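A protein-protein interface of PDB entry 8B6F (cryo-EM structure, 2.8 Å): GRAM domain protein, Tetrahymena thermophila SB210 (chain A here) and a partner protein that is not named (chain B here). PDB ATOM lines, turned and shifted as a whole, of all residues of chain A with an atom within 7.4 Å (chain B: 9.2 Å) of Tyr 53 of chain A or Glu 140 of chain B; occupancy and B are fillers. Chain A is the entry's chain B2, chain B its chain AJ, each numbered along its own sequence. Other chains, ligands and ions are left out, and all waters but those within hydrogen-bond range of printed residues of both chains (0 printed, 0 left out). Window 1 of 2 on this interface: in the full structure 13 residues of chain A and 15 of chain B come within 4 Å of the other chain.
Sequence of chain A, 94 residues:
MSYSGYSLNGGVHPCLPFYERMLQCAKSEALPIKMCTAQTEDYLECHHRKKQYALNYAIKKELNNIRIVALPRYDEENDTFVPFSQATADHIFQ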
ATOM      1  N   GLU A  45     -18.133 -26.202  14.772  1.00  0.00           N
ATOM      2  CA  GLU A  45     -17.919 -24.761  14.759  1.00  0.00           C
ATOM      3  C   GLU A  45     -17.123 -24.343  13.533  1.00  0.00           C
ATOM      4  O   GLU A  45     -17.487 -23.383  12.843  1.00  0.00           O
ATOM      5  CB  GLU A  45     -17.210 -24.331  16.044  1.00  0.00           C
ATOM      6  CG  GLU A  45     -16.860 -22.853  16.095  1.00  0.00           C
ATOM      7  CD  GLU A  45     -18.062 -21.962  15.879  1.00  0.00           C
ATOM      8  OE1 GLU A  45     -19.199 -22.427  16.101  1.00  0.00           O
ATOM      9  OE2 GLU A  45     -17.871 -20.796  15.480  1.00  0.00           O
ATOM     10  N   HIS A  48     -19.782 -24.704  10.541  1.00  0.00           N
ATOM     11  CA  HIS A  48     -20.974 -23.866  10.469  1.00  0.00           C
ATOM     12  C   HIS A  48     -20.716 -22.414  10.842  1.00  0.00           C
ATOM     13  O   HIS A  48     -21.345 -21.517  10.273  1.00  0.00           O
ATOM     14  CB  HIS A  48     -22.071 -24.425  11.381  1.00  0.00           C
ATOM     15  CG  HIS A  48     -22.696 -25.684  10.872  1.00  0.00           C
ATOM     16  ND1 HIS A  48     -23.525 -25.709   9.771  1.00  0.00           N
ATOM     17  CD2 HIS A  48     -22.626 -26.960  11.318  1.00  0.00           C
ATOM     18  CE1 HIS A  48     -23.931 -26.947   9.557  1.00  0.00           C
ATOM     19  NE2 HIS A  48     -23.400 -27.726  10.481  1.00  0.00           N
ATOM     20  N   ARG A  49     -19.823 -22.161  11.799  1.00  0.00           N
ATOM     21  CA  ARG A  49     -19.496 -20.808  12.241  1.00  0.00           C
ATOM     22  C   ARG A  49     -20.675 -20.147  12.949  1.00  0.00           C
ATOM     23  O   ARG A  49     -20.867 -18.935  12.850  1.00  0.00           O
ATOM     24  CB  ARG A  49     -19.014 -19.939  11.075  1.00  0.00           C
ATOM     25  CG  ARG A  49     -17.716 -20.428  10.457  1.00  0.00           C
ATOM     26  CD  ARG A  49     -17.651 -20.134   8.970  1.00  0.00           C
ATOM     27  NE  ARG A  49     -18.517 -21.018   8.200  1.00  0.00           N
ATOM     28  CZ  ARG A  49     -18.646 -20.978   6.882  1.00  0.00           C
ATOM     29  NH1 ARG A  49     -17.980 -20.103   6.149  1.00  0.00           N
ATOM     30  NH2 ARG A  49     -19.463 -21.838   6.284  1.00  0.00           N
ATOM     31  N   LYS A  50     -21.462 -20.939  13.678  1.00  0.00           N
ATOM     32  CA  LYS A  50     -22.605 -20.393  14.402  1.00  0.00           C
ATOM     33  C   LYS A  50     -22.159 -19.399  15.466  1.00  0.00           C
ATOM     34  O   LYS A  50     -22.767 -18.334  15.626  1.00  0.00           O
ATOM     35  CB  LYS A  50     -23.411 -21.528  15.034  1.00  0.00           C
ATOM     36  CG  LYS A  50     -24.595 -21.073  15.879  1.00  0.00           C
ATOM     37  CD  LYS A  50     -25.195 -22.242  16.640  1.00  0.00           C
ATOM     38  CE  LYS A  50     -26.255 -21.781  17.625  1.00  0.00           C
ATOM     39  NZ  LYS A  50     -26.774 -22.910  18.446  1.00  0.00           N
ATOM     40  N   LYS A  51     -21.099 -19.728  16.206  1.00  0.00           N
ATOM     41  CA  LYS A  51     -20.665 -18.865  17.299  1.00  0.00           C
ATOM     42  C   LYS A  51     -20.218 -17.502  16.787  1.00  0.00           C
ATOM     43  O   LYS A  51     -20.493 -16.475  17.417  1.00  0.00           O
ATOM     44  CB  LYS A  51     -19.546 -19.543  18.086  1.00  0.00           C
ATOM     45  CG  LYS A  51     -19.985 -20.824  18.774  1.00  0.00           C
ATOM     46  CD  LYS A  51     -18.880 -21.393  19.645  1.00  0.00           C
ATOM     47  CE  LYS A  51     -19.357 -22.621  20.403  1.00  0.00           C
ATOM     48  NZ  LYS A  51     -18.301 -23.164  21.303  1.00  0.00           N
ATOM     49  N   GLN A  52     -19.519 -17.468  15.652  1.00  0.00           N
ATOM     50  CA  GLN A  52     -19.111 -16.187  15.090  1.00  0.00           C
ATOM     51  C   GLN A  52     -20.318 -15.365  14.659  1.00  0.00           C
ATOM     52  O   GLN A  52     -20.336 -14.141  14.831  1.00  0.00           O
ATOM     53  CB  GLN A  52     -18.169 -16.401  13.911  1.00  0.00           C
ATOM     54  CG  GLN A  52     -17.518 -15.120  13.418  1.00  0.00           C
ATOM     55  CD  GLN A  52     -16.560 -14.524  14.423  1.00  0.00           C
ATOM     56  OE1 GLN A  52     -16.180 -15.173  15.396  1.00  0.00           O
ATOM     57  NE2 GLN A  52     -16.158 -13.280  14.191  1.00  0.00           N
ATOM     58  N   TYR A  53     -21.341 -16.016  14.104  1.00  0.00           N
ATOM     59  CA  TYR A  53     -22.552 -15.291  13.736  1.00  0.00           C
ATOM     60  C   TYR A  53     -23.240 -14.717  14.967  1.00  0.00           C
ATOM     61  O   TYR A  53     -23.745 -13.590  14.935  1.00  0.00           O
ATOM     62  CB  TYR A  53     -23.503 -16.207  12.968  1.00  0.00           C
ATOM     63  CG  TYR A  53     -23.136 -16.385  11.514  1.00  0.00           C
ATOM     64  CD1 TYR A  53     -23.230 -15.325  10.622  1.00  0.00           C
ATOM     65  CD2 TYR A  53     -22.709 -17.611  11.032  1.00  0.00           C
ATOM     66  CE1 TYR A  53     -22.901 -15.484   9.292  1.00  0.00           C
ATOM     67  CE2 TYR A  53     -22.376 -17.778   9.704  1.00  0.00           C
ATOM     68  CZ  TYR A  53     -22.474 -16.711   8.838  1.00  0.00           C
ATOM     69  OH  TYR A  53     -22.147 -16.870   7.514  1.00  0.00           O
ATOM     70  N   ALA A  54     -23.274 -15.479  16.060  1.00  0.00           N
ATOM     71  CA  ALA A  54     -23.843 -14.956  17.296  1.00  0.00           C
ATOM     72  C   ALA A  54     -23.046 -13.759  17.796  1.00  0.00           C
ATOM     73  O   ALA A  54     -23.623 -12.761  18.244  1.00  0.00           O
ATOM     74  CB  ALA A  54     -23.891 -16.053  18.357  1.00  0.00           C
ATOM     75  N   LEU A  55     -21.716 -13.841  17.733  1.00  0.00           N
ATOM     76  CA  LEU A  55     -20.886 -12.710  18.129  1.00  0.00           C
ATOM     77  C   LEU A  55     -21.165 -11.494  17.257  1.00  0.00           C
ATOM     78  O   LEU A  55     -21.249 -10.368  17.756  1.00  0.00           O
ATOM     79  CB  LEU A  55     -19.409 -13.096  18.060  1.00  0.00           C
ATOM     80  CG  LEU A  55     -18.405 -11.960  18.264  1.00  0.00           C
ATOM     81  CD1 LEU A  55     -18.632 -11.264  19.592  1.00  0.00           C
ATOM     82  CD2 LEU A  55     -16.988 -12.490  18.175  1.00  0.00           C
ATOM     83  N   ASN A  56     -21.313 -11.705  15.948  1.00  0.00           N
ATOM     84  CA  ASN A  56     -21.601 -10.595  15.045  1.00  0.00           C
ATOM     85  C   ASN A  56     -22.959  -9.979  15.352  1.00  0.00           C
ATOM     86  O   ASN A  56     -23.121  -8.755  15.303  1.00  0.00           O
ATOM     87  CB  ASN A  56     -21.545 -11.071  13.595  1.00  0.00           C
ATOM     88  CG  ASN A  56     -20.162 -11.531  13.188  1.00  0.00           C
ATOM     89  OD1 ASN A  56     -19.161 -11.101  13.757  1.00  0.00           O
ATOM     90  ND2 ASN A  56     -20.100 -12.411  12.197  1.00  0.00           N
ATOM     91  N   TYR A  57     -23.947 -10.814  15.671  1.00  0.00           N
ATOM     92  CA  TYR A  57     -25.259 -10.301  16.049  1.00  0.00           C
ATOM     93  C   TYR A  57     -25.162  -9.435  17.297  1.00  0.00           C
ATOM     94  O   TYR A  57     -25.736  -8.342  17.357  1.00  0.00           O
ATOM     95  CB  TYR A  57     -26.219 -11.472  16.265  1.00  0.00           C
ATOM     96  CG  TYR A  57     -27.597 -11.082  16.748  1.00  0.00           C
ATOM     97  CD1 TYR A  57     -28.597 -10.736  15.850  1.00  0.00           C
ATOM     98  CD2 TYR A  57     -27.904 -11.091  18.102  1.00  0.00           C
ATOM     99  CE1 TYR A  57     -29.862 -10.392  16.288  1.00  0.00           C
ATOM    100  CE2 TYR A  57     -29.165 -10.749  18.550  1.00  0.00           C
ATOM    101  CZ  TYR A  57     -30.139 -10.400  17.639  1.00  0.00           C
ATOM    102  OH  TYR A  57     -31.395 -10.060  18.084  1.00  0.00           O
ATOM    103  N   ALA A  58     -24.440  -9.912  18.312  1.00  0.00           N
ATOM    104  CA  ALA A  58     -24.270  -9.130  19.532  1.00  0.00           C
ATOM    105  C   ALA A  58     -23.543  -7.820  19.253  1.00  0.00           C
ATOM    106  O   ALA A  58     -23.917  -6.769  19.784  1.00  0.00           O
ATOM    107  CB  ALA A  58     -23.513  -9.951  20.575  1.00  0.00           C
ATOM    108  N   ILE A  59     -22.507  -7.864  18.415  1.00  0.00           N
ATOM    109  CA  ILE A  59     -21.744  -6.660  18.096  1.00  0.00           C
ATOM    110  C   ILE A  59     -22.607  -5.663  17.335  1.00  0.00           C
ATOM    111  O   ILE A  59     -22.497  -4.449  17.540  1.00  0.00           O
ATOM    112  CB  ILE A  59     -20.472  -7.031  17.311  1.00  0.00           C
ATOM    113  CG1 ILE A  59     -19.479  -7.762  18.219  1.00  0.00           C
ATOM    114  CG2 ILE A  59     -19.828  -5.791  16.687  1.00  0.00           C
ATOM    115  CD1 ILE A  59     -18.845  -6.897  19.290  1.00  0.00           C
ATOM    116  N   LEU B  30     -32.045  -3.143   4.251  1.00  0.00           N
ATOM    117  CA  LEU B  30     -30.664  -3.506   3.953  1.00  0.00           C
ATOM    118  C   LEU B  30     -30.636  -4.379   2.706  1.00  0.00           C
ATOM    119  O   LEU B  30     -31.162  -5.497   2.714  1.00  0.00           O
ATOM    120  CB  LEU B  30     -30.024  -4.240   5.132  1.00  0.00           C
ATOM    121  CG  LEU B  30     -29.889  -3.445   6.430  1.00  0.00           C
ATOM    122  CD1 LEU B  30     -29.336  -4.325   7.539  1.00  0.00           C
ATOM    123  CD2 LEU B  30     -29.006  -2.225   6.231  1.00  0.00           C
ATOM    124  N   TYR B  76     -21.521 -14.033  -7.726  1.00  0.00           N
ATOM    125  CA  TYR B  76     -20.909 -14.844  -6.684  1.00  0.00           C
ATOM    126  C   TYR B  76     -19.508 -15.312  -7.053  1.00  0.00           C
ATOM    127  O   TYR B  76     -18.862 -15.980  -6.240  1.00  0.00           O
ATOM    128  CB  TYR B  76     -21.796 -16.052  -6.383  1.00  0.00           C
ATOM    129  CG  TYR B  76     -21.860 -16.413  -4.919  1.00  0.00           C
ATOM    130  CD1 TYR B  76     -22.615 -15.657  -4.033  1.00  0.00           C
ATOM    131  CD2 TYR B  76     -21.177 -17.513  -4.426  1.00  0.00           C
ATOM    132  CE1 TYR B  76     -22.683 -15.985  -2.696  1.00  0.00           C
ATOM    133  CE2 TYR B  76     -21.238 -17.848  -3.091  1.00  0.00           C
ATOM    134  CZ  TYR B  76     -21.992 -17.081  -2.232  1.00  0.00           C
ATOM    135  OH  TYR B  76     -22.052 -17.414  -0.900  1.00  0.00           O
ATOM    136  N   ASP B 136     -32.896 -21.151   6.026  1.00  0.00           N
ATOM    137  CA  ASP B 136     -31.712 -20.374   6.370  1.00  0.00           C
ATOM    138  C   ASP B 136     -31.666 -20.142   7.873  1.00  0.00           C
ATOM    139  O   ASP B 136     -32.545 -19.485   8.437  1.00  0.00           O
ATOM    140  CB  ASP B 136     -31.730 -19.047   5.616  1.00  0.00           C
ATOM    141  CG  ASP B 136     -30.464 -18.248   5.815  1.00  0.00           C
ATOM    142  OD1 ASP B 136     -29.372 -18.798   5.572  1.00  0.00           O
ATOM    143  OD2 ASP B 136     -30.558 -17.067   6.204  1.00  0.00           O
ATOM    144  N   TYR B 137     -30.634 -20.683   8.521  1.00  0.00           N
ATOM    145  CA  TYR B 137     -30.569 -20.663   9.978  1.00  0.00           C
ATOM    146  C   TYR B 137     -30.080 -19.315  10.496  1.00  0.00           C
ATOM    147  O   TYR B 137     -30.820 -18.593  11.174  1.00  0.00           O
ATOM    148  CB  TYR B 137     -29.655 -21.795  10.466  1.00  0.00           C
ATOM    149  CG  TYR B 137     -29.717 -22.082  11.955  1.00  0.00           C
ATOM    150  CD1 TYR B 137     -30.543 -21.352  12.802  1.00  0.00           C
ATOM    151  CD2 TYR B 137     -28.940 -23.088  12.512  1.00  0.00           C
ATOM    152  CE1 TYR B 137     -30.592 -21.618  14.156  1.00  0.00           C
ATOM    153  CE2 TYR B 137     -28.983 -23.361  13.864  1.00  0.00           C
ATOM    154  CZ  TYR B 137     -29.811 -22.622  14.682  1.00  0.00           C
ATOM    155  OH  TYR B 137     -29.857 -22.889  16.029  1.00  0.00           O
ATOM    156  N   PHE B 138     -28.831 -18.958  10.185  1.00  0.00           N
ATOM    157  CA  PHE B 138     -28.236 -17.751  10.746  1.00  0.00           C
ATOM    158  C   PHE B 138     -27.434 -16.950   9.727  1.00  0.00           C
ATOM    159  O   PHE B 138     -26.690 -16.045  10.125  1.00  0.00           O
ATOM    160  CB  PHE B 138     -27.340 -18.108  11.940  1.00  0.00           C
ATOM    161  CG  PHE B 138     -26.512 -19.340  11.730  1.00  0.00           C
ATOM    162  CD1 PHE B 138     -25.444 -19.332  10.851  1.00  0.00           C
ATOM    163  CD2 PHE B 138     -26.796 -20.506  12.420  1.00  0.00           C
ATOM    164  CE1 PHE B 138     -24.678 -20.463  10.658  1.00  0.00           C
ATOM    165  CE2 PHE B 138     -26.035 -21.643  12.232  1.00  0.00           C
ATOM    166  CZ  PHE B 138     -24.974 -21.621  11.350  1.00  0.00           C
ATOM    167  N   SER B 139     -27.557 -17.241   8.436  1.00  0.00           N
ATOM    168  CA  SER B 139     -26.825 -16.479   7.434  1.00  0.00           C
ATOM    169  C   SER B 139     -27.200 -15.006   7.520  1.00  0.00           C
ATOM    170  O   SER B 139     -28.365 -14.653   7.717  1.00  0.00           O
ATOM    171  CB  SER B 139     -27.124 -17.013   6.036  1.00  0.00           C
ATOM    172  OG  SER B 139     -26.289 -16.391   5.078  1.00  0.00           O
ATOM    173  N   GLU B 140     -26.200 -14.143   7.372  1.00  0.00           N
ATOM    174  CA  GLU B 140     -26.370 -12.708   7.542  1.00  0.00           C
ATOM    175  C   GLU B 140     -26.187 -11.995   6.210  1.00  0.00           C
ATOM    176  O   GLU B 140     -25.278 -12.317   5.441  1.00  0.00           O
ATOM    177  CB  GLU B 140     -25.371 -12.164   8.566  1.00  0.00           C
ATOM    178  CG  GLU B 140     -23.929 -12.196   8.096  1.00  0.00           C
ATOM    179  CD  GLU B 140     -22.949 -11.902   9.212  1.00  0.00           C
ATOM    180  OE1 GLU B 140     -23.335 -12.032  10.391  1.00  0.00           O
ATOM    181  OE2 GLU B 140     -21.795 -11.537   8.910  1.00  0.00           O
ATOM    182  N   LEU B 141     -27.061 -11.028   5.947  1.00  0.00           N
ATOM    183  CA  LEU B 141     -26.967 -10.237   4.731  1.00  0.00           C
ATOM    184  C   LEU B 141     -25.718  -9.367   4.745  1.00  0.00           C
ATOM    185  O   LEU B 141     -25.182  -9.024   5.801  1.00  0.00           O
ATOM    186  CB  LEU B 141     -28.196  -9.340   4.578  1.00  0.00           C
ATOM    187  CG  LEU B 141     -29.481  -9.973   4.053  1.00  0.00           C
ATOM    188  CD1 LEU B 141     -30.650  -9.027   4.253  1.00  0.00           C
ATOM    189  CD2 LEU B 141     -29.331 -10.330   2.588  1.00  0.00           C
ATOM    190  N   GLU B 142     -25.249  -9.019   3.551  1.00  0.00           N
ATOM    191  CA  GLU B 142     -24.285  -7.940   3.428  1.00  0.00           C
ATOM    192  C   GLU B 142     -24.932  -6.640   3.889  1.00  0.00           C
ATOM    193  O   GLU B 142     -26.137  -6.431   3.720  1.00  0.00           O
ATOM    194  CB  GLU B 142     -23.797  -7.818   1.985  1.00  0.00           C
ATOM    195  CG  GLU B 142     -23.080  -9.060   1.473  1.00  0.00           C
ATOM    196  CD  GLU B 142     -22.785  -8.996  -0.014  1.00  0.00           C
ATOM    197  OE1 GLU B 142     -23.198  -8.015  -0.663  1.00  0.00           O
ATOM    198  OE2 GLU B 142     -22.143  -9.929  -0.535  1.00  0.00           O
ATOM    199  N   LEU B 143     -24.127  -5.767   4.485  1.00  0.00           N
ATOM    200  CA  LEU B 143     -24.550  -4.545   5.161  1.00  0.00           C
ATOM    201  C   LEU B 143     -25.084  -4.851   6.555  1.00  0.00           C
ATOM    202  O   LEU B 143     -25.469  -3.919   7.269  1.00  0.00           O
ATOM    203  CB  LEU B 143     -25.624  -3.762   4.386  1.00  0.00           C
ATOM    204  CG  LEU B 143     -25.275  -3.394   2.945  1.00  0.00           C
ATOM    205  CD1 LEU B 143     -26.509  -2.932   2.198  1.00  0.00           C
ATOM    206  CD2 LEU B 143     -24.200  -2.320   2.929  1.00  0.00           C
ATOM    207  N   PHE B 144     -25.128  -6.118   6.967  1.00  0.00           N
ATOM    208  CA  PHE B 144     -25.508  -6.435   8.338  1.00  0.00           C
ATOM    209  C   PHE B 144     -24.536  -5.803   9.324  1.00  0.00           C
ATOM    210  O   PHE B 144     -24.949  -5.246  10.347  1.00  0.00           O
ATOM    211  CB  PHE B 144     -25.562  -7.951   8.520  1.00  0.00           C
ATOM    212  CG  PHE B 144     -25.895  -8.386   9.916  1.00  0.00           C
ATOM    213  CD1 PHE B 144     -27.209  -8.458  10.337  1.00  0.00           C
ATOM    214  CD2 PHE B 144     -24.890  -8.737  10.801  1.00  0.00           C
ATOM    215  CE1 PHE B 144     -27.517  -8.864  11.620  1.00  0.00           C
ATOM    216  CE2 PHE B 144     -25.191  -9.144  12.083  1.00  0.00           C
ATOM    217  CZ  PHE B 144     -26.506  -9.208  12.493  1.00  0.00           C
ATOM    218  N   LEU B 145     -23.247  -5.875   9.030  1.00  0.00           N
ATOM    219  CA  LEU B 145     -22.195  -5.209   9.778  1.00  0.00           C
ATOM    220  C   LEU B 145     -21.321  -4.432   8.810  1.00  0.00           C
ATOM    221  O   LEU B 145     -21.283  -4.739   7.613  1.00  0.00           O
ATOM    222  CB  LEU B 145     -21.332  -6.209  10.562  1.00  0.00           C
ATOM    223  CG  LEU B 145     -21.894  -6.743  11.879  1.00  0.00           C
ATOM    224  CD1 LEU B 145     -20.957  -7.777  12.471  1.00  0.00           C
ATOM    225  CD2 LEU B 145     -22.122  -5.612  12.870  1.00  0.00           C
ATOM    226  N   PRO B 146     -20.612  -3.413   9.290  1.00  0.00           N
ATOM    227  CA  PRO B 146     -19.730  -2.656   8.395  1.00  0.00           C
ATOM    228  C   PRO B 146     -18.690  -3.562   7.755  1.00  0.00           C
ATOM    229  O   PRO B 146     -18.172  -4.488   8.382  1.00  0.00           O
ATOM    230  CB  PRO B 146     -19.084  -1.621   9.321  1.00  0.00           C
ATOM    231  CG  PRO B 146     -20.021  -1.497  10.466  1.00  0.00           C
ATOM    232  CD  PRO B 146     -20.626  -2.851  10.651  1.00  0.00           C
ATOM    233  N   LEU B 149     -15.132  -4.239   9.432  1.00  0.00           N
ATOM    234  CA  LEU B 149     -14.865  -5.228  10.469  1.00  0.00           C
ATOM    235  C   LEU B 149     -14.297  -6.517   9.892  1.00  0.00           C
ATOM    236  O   LEU B 149     -13.515  -7.198  10.564  1.00  0.00           O
ATOM    237  CB  LEU B 149     -16.142  -5.524  11.257  1.00  0.00           C
ATOM    238  CG  LEU B 149     -16.776  -4.344  11.997  1.00  0.00           C
ATOM    239  CD1 LEU B 149     -17.988  -4.808  12.784  1.00  0.00           C
ATOM    240  CD2 LEU B 149     -15.781  -3.655  12.915  1.00  0.00           C
ATOM    241  N   SER B 150     -14.676  -6.872   8.667  1.00  0.00           N
ATOM    242  CA  SER B 150     -14.151  -8.067   8.024  1.00  0.00           C
ATOM    243  C   SER B 150     -12.733  -7.806   7.532  1.00  0.00           C
ATOM    244  O   SER B 150     -12.466  -6.780   6.901  1.00  0.00           O
ATOM    245  CB  SER B 150     -15.051  -8.481   6.861  1.00  0.00           C
ATOM    246  OG  SER B 150     -14.566  -9.655   6.234  1.00  0.00           O
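O of His 48 of chain A touches CE1 of Phe 138 of chain B, at 3.5 Å. Lys 50 of chain A touches Tyr 137 of chain B (NZ to OH, 3.9 Å). CE2 of Phe 138 of chain B touches CB of Lys 50 of chain A, 3.8 Å away. Tyr 53 of chain A touches Phe 138 of chain B. Tyr 53 of chain A touches Glu 140 of chain B (CD1 to OE1, 3.3 Å). Asn 56 of chain A touches Glu 140 of chain B (ND2 to OE1, 3.7 Å). O of Asn 56 of chain A touches CE2 of Phe 144 of chain B, at 3.8 Å. Asn 56 of chain A touches Leu 145 of chain B (CB to CD1, 3.5 Å). Phe 144 of chain B touches Tyr 57 of chain A (CZ to CA, 3.9 Å).
Hydrophobic or aromatic side chains of chain A within 4 Å of the printed part of chain B: Tyr 53. Among the printed residues, 9 pairs touch across the chains.
The backbone carbonyl oxygen (O) of Gln 52 of chain A sits close to the side-chain amide nitrogen (ND2) of Asn 56 of chain A (3.2 Å).
Of the printed residues of chain B, Tyr 53 of chain A touches Phe 138 and Glu 140. Glu 140 of chain B touches just these residues of chain A: Tyr 53 and Asn 56. No residue of chain B comes within 4 Å of Ala 54 of chain A. Printed residues of chain A within 4 Å of Phe 144 of chain B: Asn 56 (3.8 Å) and Tyr 57 (3.9 Å). Printed residues of chain A within 4 Å of Tyr 137 of chain B: Lys 50. Printed residues of chain B within 4 Å of Tyr 57 of chain A: Phe 144. Printed residues of chain B within 4 Å of Lys 50 of chain A: Tyr 137 and Phe 138. Ala 58 of chain A touches none of the printed residues of chain B. The nearest residue of chain A that does not touch Glu 140 of chain B is Tyr 57 of chain A (5.5 Å). The nearest printed residue of chain A that does not touch Tyr 137 of chain B is His 48 of chain A (6.6 Å).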
